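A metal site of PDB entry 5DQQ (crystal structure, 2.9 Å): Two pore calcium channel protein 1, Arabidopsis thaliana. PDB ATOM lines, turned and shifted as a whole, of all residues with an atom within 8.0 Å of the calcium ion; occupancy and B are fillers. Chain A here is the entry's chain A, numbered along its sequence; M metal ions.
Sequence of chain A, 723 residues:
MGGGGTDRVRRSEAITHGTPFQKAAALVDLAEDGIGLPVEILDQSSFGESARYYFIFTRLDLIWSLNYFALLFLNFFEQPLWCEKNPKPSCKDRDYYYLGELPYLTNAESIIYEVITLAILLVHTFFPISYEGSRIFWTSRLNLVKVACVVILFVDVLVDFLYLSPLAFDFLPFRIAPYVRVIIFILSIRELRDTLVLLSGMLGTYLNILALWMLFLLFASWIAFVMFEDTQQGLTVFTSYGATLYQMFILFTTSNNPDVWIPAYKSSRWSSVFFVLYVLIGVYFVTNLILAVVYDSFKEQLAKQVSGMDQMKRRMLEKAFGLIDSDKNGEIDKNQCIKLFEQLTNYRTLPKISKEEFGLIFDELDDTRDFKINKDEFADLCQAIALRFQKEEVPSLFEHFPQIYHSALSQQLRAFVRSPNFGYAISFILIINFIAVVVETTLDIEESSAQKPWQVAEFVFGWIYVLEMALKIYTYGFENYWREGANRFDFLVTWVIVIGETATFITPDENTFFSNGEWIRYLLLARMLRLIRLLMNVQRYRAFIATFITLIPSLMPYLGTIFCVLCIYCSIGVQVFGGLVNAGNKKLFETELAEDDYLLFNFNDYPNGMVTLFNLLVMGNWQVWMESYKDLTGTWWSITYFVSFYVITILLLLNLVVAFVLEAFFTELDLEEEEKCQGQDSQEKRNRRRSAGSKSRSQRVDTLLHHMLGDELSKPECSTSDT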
ATOM      1  N   PHE A 321      25.156  19.270 -35.268  1.00  0.00           N
ATOM      2  CA  PHE A 321      25.400  20.216 -34.192  1.00  0.00           C
ATOM      3  C   PHE A 321      26.151  19.559 -33.041  1.00  0.00           C
ATOM      4  O   PHE A 321      27.188  20.062 -32.596  1.00  0.00           O
ATOM      5  CB  PHE A 321      24.090  20.816 -33.687  1.00  0.00           C
ATOM      6  CG  PHE A 321      24.251  21.605 -32.406  1.00  0.00           C
ATOM      7  CD1 PHE A 321      24.216  20.966 -31.173  1.00  0.00           C
ATOM      8  CD2 PHE A 321      24.465  22.972 -32.441  1.00  0.00           C
ATOM      9  CE1 PHE A 321      24.378  21.676 -30.008  1.00  0.00           C
ATOM     10  CE2 PHE A 321      24.627  23.683 -31.276  1.00  0.00           C
ATOM     11  CZ  PHE A 321      24.581  23.039 -30.062  1.00  0.00           C
ATOM     12  N   ILE A 324      29.631  19.448 -33.577  1.00  0.00           N
ATOM     13  CA  ILE A 324      30.331  20.718 -33.438  1.00  0.00           C
ATOM     14  C   ILE A 324      30.501  21.071 -31.968  1.00  0.00           C
ATOM     15  O   ILE A 324      31.514  21.667 -31.563  1.00  0.00           O
ATOM     16  CB  ILE A 324      29.589  21.835 -34.204  1.00  0.00           C
ATOM     17  CG1 ILE A 324      30.599  22.846 -34.764  1.00  0.00           C
ATOM     18  CG2 ILE A 324      28.587  22.537 -33.302  1.00  0.00           C
ATOM     19  CD1 ILE A 324      29.986  23.844 -35.742  1.00  0.00           C
ATOM     20  N   ASP A 325      29.524  20.718 -31.135  1.00  0.00           N
ATOM     21  CA  ASP A 325      29.524  21.090 -29.725  1.00  0.00           C
ATOM     22  C   ASP A 325      30.319  20.035 -28.953  1.00  0.00           C
ATOM     23  O   ASP A 325      29.773  19.062 -28.439  1.00  0.00           O
ATOM     24  CB  ASP A 325      28.099  21.206 -29.210  1.00  0.00           C
ATOM     25  CG  ASP A 325      28.057  21.538 -27.731  1.00  0.00           C
ATOM     26  OD1 ASP A 325      28.706  22.520 -27.332  1.00  0.00           O
ATOM     27  OD2 ASP A 325      27.365  20.817 -26.984  1.00  0.00           O
ATOM     28  N   SER A 326      31.625  20.257 -28.859  1.00  0.00           N
ATOM     29  CA  SER A 326      32.482  19.291 -28.182  1.00  0.00           C
ATOM     30  C   SER A 326      32.286  19.340 -26.665  1.00  0.00           C
ATOM     31  O   SER A 326      32.325  18.306 -25.999  1.00  0.00           O
ATOM     32  CB  SER A 326      33.941  19.545 -28.541  1.00  0.00           C
ATOM     33  OG  SER A 326      34.259  20.924 -28.439  1.00  0.00           O
ATOM     34  N   ASP A 327      32.064  20.535 -26.115  1.00  0.00           N
ATOM     35  CA  ASP A 327      32.036  20.678 -24.662  1.00  0.00           C
ATOM     36  C   ASP A 327      30.817  20.003 -24.040  1.00  0.00           C
ATOM     37  O   ASP A 327      30.849  19.629 -22.872  1.00  0.00           O
ATOM     38  CB  ASP A 327      32.098  22.158 -24.286  1.00  0.00           C
ATOM     39  CG  ASP A 327      31.422  23.042 -25.304  1.00  0.00           C
ATOM     40  OD1 ASP A 327      31.161  22.553 -26.430  1.00  0.00           O
ATOM     41  OD2 ASP A 327      31.165  24.223 -24.992  1.00  0.00           O
ATOM     42  N   LYS A 328      29.741  19.843 -24.805  1.00  0.00           N
ATOM     43  CA  LYS A 328      28.485  19.216 -24.403  1.00  0.00           C
ATOM     44  C   LYS A 328      27.549  20.167 -23.664  1.00  0.00           C
ATOM     45  O   LYS A 328      26.429  19.755 -23.331  1.00  0.00           O
ATOM     46  CB  LYS A 328      28.695  17.981 -23.518  1.00  0.00           C
ATOM     47  CG  LYS A 328      28.864  16.674 -24.255  1.00  0.00           C
ATOM     48  CD  LYS A 328      28.751  15.513 -23.279  1.00  0.00           C
ATOM     49  CE  LYS A 328      28.988  14.173 -23.963  1.00  0.00           C
ATOM     50  NZ  LYS A 328      28.863  13.044 -23.010  1.00  0.00           N
ATOM     51  N   ASN A 329      27.946  21.412 -23.400  1.00  0.00           N
ATOM     52  CA  ASN A 329      27.038  22.338 -22.737  1.00  0.00           C
ATOM     53  C   ASN A 329      25.711  22.495 -23.474  1.00  0.00           C
ATOM     54  O   ASN A 329      24.719  22.877 -22.848  1.00  0.00           O
ATOM     55  CB  ASN A 329      27.701  23.710 -22.584  1.00  0.00           C
ATOM     56  CG  ASN A 329      28.504  24.105 -23.820  1.00  0.00           C
ATOM     57  OD1 ASN A 329      28.589  23.349 -24.783  1.00  0.00           O
ATOM     58  ND2 ASN A 329      29.095  25.290 -23.780  1.00  0.00           N
ATOM     59  N   GLY A 330      25.666  22.190 -24.765  1.00  0.00           N
ATOM     60  CA  GLY A 330      24.462  22.355 -25.553  1.00  0.00           C
ATOM     61  C   GLY A 330      24.403  23.623 -26.384  1.00  0.00           C
ATOM     62  O   GLY A 330      23.344  23.910 -26.955  1.00  0.00           O
ATOM     63  N   GLU A 331      25.495  24.372 -26.462  1.00  0.00           N
ATOM     64  CA  GLU A 331      25.537  25.608 -27.229  1.00  0.00           C
ATOM     65  C   GLU A 331      26.896  25.707 -27.913  1.00  0.00           C
ATOM     66  O   GLU A 331      27.856  25.058 -27.502  1.00  0.00           O
ATOM     67  CB  GLU A 331      25.271  26.825 -26.339  1.00  0.00           C
ATOM     68  CG  GLU A 331      24.259  26.543 -25.227  1.00  0.00           C
ATOM     69  CD  GLU A 331      23.507  27.772 -24.775  1.00  0.00           C
ATOM     70  OE1 GLU A 331      23.799  28.870 -25.276  1.00  0.00           O
ATOM     71  OE2 GLU A 331      22.596  27.630 -23.918  1.00  0.00           O
ATOM     72  N   ILE A 332      26.965  26.523 -28.963  1.00  0.00           N
ATOM     73  CA  ILE A 332      28.151  26.617 -29.813  1.00  0.00           C
ATOM     74  C   ILE A 332      28.666  28.047 -29.765  1.00  0.00           C
ATOM     75  O   ILE A 332      27.882  29.006 -29.867  1.00  0.00           O
ATOM     76  CB  ILE A 332      27.840  26.185 -31.246  1.00  0.00           C
ATOM     77  N   ASP A 333      29.991  28.194 -29.616  1.00  0.00           N
ATOM     78  CA  ASP A 333      30.593  29.507 -29.480  1.00  0.00           C
ATOM     79  C   ASP A 333      30.561  30.260 -30.808  1.00  0.00           C
ATOM     80  O   ASP A 333      30.495  29.657 -31.887  1.00  0.00           O
ATOM     81  CB  ASP A 333      32.049  29.379 -29.014  1.00  0.00           C
ATOM     82  CG  ASP A 333      32.235  28.258 -28.019  1.00  0.00           C
ATOM     83  OD1 ASP A 333      31.241  27.812 -27.422  1.00  0.00           O
ATOM     84  OD2 ASP A 333      33.397  27.811 -27.840  1.00  0.00           O
ATOM     85  N   LYS A 334      30.630  31.590 -30.726  1.00  0.00           N
ATOM     86  CA  LYS A 334      30.777  32.388 -31.940  1.00  0.00           C
ATOM     87  C   LYS A 334      31.944  31.882 -32.767  1.00  0.00           C
ATOM     88  O   LYS A 334      31.794  31.583 -33.956  1.00  0.00           O
ATOM     89  CB  LYS A 334      30.967  33.865 -31.594  1.00  0.00           C
ATOM     90  CG  LYS A 334      31.501  34.683 -32.757  1.00  0.00           C
ATOM     91  CD  LYS A 334      32.017  36.033 -32.302  1.00  0.00           C
ATOM     92  CE  LYS A 334      33.464  36.241 -32.729  1.00  0.00           C
ATOM     93  NZ  LYS A 334      34.389  35.260 -32.084  1.00  0.00           N
ATOM     94  N   GLN A 336      33.234  29.076 -32.674  1.00  0.00           N
ATOM     95  CA  GLN A 336      32.949  27.715 -33.103  1.00  0.00           C
ATOM     96  C   GLN A 336      31.998  27.693 -34.288  1.00  0.00           C
ATOM     97  O   GLN A 336      32.145  26.874 -35.198  1.00  0.00           O
ATOM     98  CB  GLN A 336      32.378  26.900 -31.939  1.00  0.00           C
ATOM     99  CG  GLN A 336      33.047  25.559 -31.718  1.00  0.00           C
ATOM    100  CD  GLN A 336      32.764  24.976 -30.344  1.00  0.00           C
ATOM    101  OE1 GLN A 336      31.796  25.353 -29.684  1.00  0.00           O
ATOM    102  NE2 GLN A 336      33.624  24.064 -29.897  1.00  0.00           N
ATOM    103  N   CYS A 337      30.997  28.584 -34.297  1.00  0.00           N
ATOM    104  CA  CYS A 337      29.987  28.560 -35.353  1.00  0.00           C
ATOM    105  C   CYS A 337      30.436  29.329 -36.602  1.00  0.00           C
ATOM    106  O   CYS A 337      29.953  29.031 -37.702  1.00  0.00           O
ATOM    107  CB  CYS A 337      28.664  29.129 -34.842  1.00  0.00           C
ATOM    108  SG  CYS A 337      27.683  27.987 -33.831  1.00  0.00           S
ATOM    109  N   PHE A 371      27.641  35.056 -27.376  1.00  0.00           N
ATOM    110  CA  PHE A 371      27.813  34.344 -28.631  1.00  0.00           C
ATOM    111  C   PHE A 371      27.530  32.847 -28.450  1.00  0.00           C
ATOM    112  O   PHE A 371      28.348  31.986 -28.788  1.00  0.00           O
ATOM    113  CB  PHE A 371      29.206  34.582 -29.199  1.00  0.00           C
ATOM    114  N   LYS A 372      26.360  32.540 -27.902  1.00  0.00           N
ATOM    115  CA  LYS A 372      25.941  31.174 -27.643  1.00  0.00           C
ATOM    116  C   LYS A 372      24.628  30.908 -28.358  1.00  0.00           C
ATOM    117  O   LYS A 372      23.626  31.586 -28.097  1.00  0.00           O
ATOM    118  CB  LYS A 372      25.818  30.907 -26.142  1.00  0.00           C
ATOM    119  CG  LYS A 372      27.149  31.023 -25.433  1.00  0.00           C
ATOM    120  CD  LYS A 372      27.051  30.810 -23.933  1.00  0.00           C
ATOM    121  CE  LYS A 372      28.371  31.189 -23.278  1.00  0.00           C
ATOM    122  NZ  LYS A 372      28.475  30.704 -21.879  1.00  0.00           N
ATOM    123  N   ILE A 373      24.642  29.931 -29.264  1.00  0.00           N
ATOM    124  CA  ILE A 373      23.467  29.511 -30.010  1.00  0.00           C
ATOM    125  C   ILE A 373      23.176  28.064 -29.643  1.00  0.00           C
ATOM    126  O   ILE A 373      24.085  27.227 -29.623  1.00  0.00           O
ATOM    127  CB  ILE A 373      23.665  29.672 -31.526  1.00  0.00           C
ATOM    128  CG1 ILE A 373      22.349  30.051 -32.207  1.00  0.00           C
ATOM    129  CG2 ILE A 373      24.239  28.392 -32.129  1.00  0.00           C
ATOM    130  CD1 ILE A 373      22.510  31.112 -33.275  1.00  0.00           C
HETATM  131 CA    CA M   1      30.128  24.734 -27.189  1.00  0.00          CA
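Asn 329 touches the calcium ion (OD1 to CA, 3.2 Å). Ile 332 touches the calcium ion. Asp 333 touches the calcium ion. Within 4 Å of the calcium ion: Asp 325, Asp 327, Asn 329, Glu 331, Ile 332, Asp 333 and Gln 336. Along chain A the residues within 4 Å of the calcium ion span positions 325 to 336.
O of Glu 331 is bound to the calcium ion, at 2.3 Å. The calcium ion is bound by OD2 of Asp 327 (2.5 Å). The calcium ion is bound by the side-chain carboxylate (OD1) of Asp 327 (2.5 Å). OD1 of Asp 325 is bound to the calcium ion, at 2.6 Å. Slightly farther from the calcium ion lies OE1 of Gln 336 (3.1 Å).
The side-chain amide oxygen (OD1) of Asn 329 lies close to the backbone carbonyl oxygen (O) of Glu 331, at 3.3 Å. OD2 of Asp 327 sits close to ND2 of Asn 329 (2.6 Å). The side-chain amide oxygen (OD1) of Asn 329 lies close to the side-chain carboxylate (OD1) of Asp 325 (2.7 Å). The side-chain carboxylate (OD2) of Asp 325 lies close to the backbone NH (N) of Lys 328. OD2 of Asp 325 lies within hydrogen-bond range of N of Gly 330 (3.1 Å). The side-chain amide oxygen of Gln 336 lies within hydrogen-bond range of the backbone NH of Asp 333 (3.4 Å). The backbone carbonyl oxygen (O) of Ile 373 is in hydrogen-bond range of the backbone NH (N) of Ile 332, 3.0 Å away.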
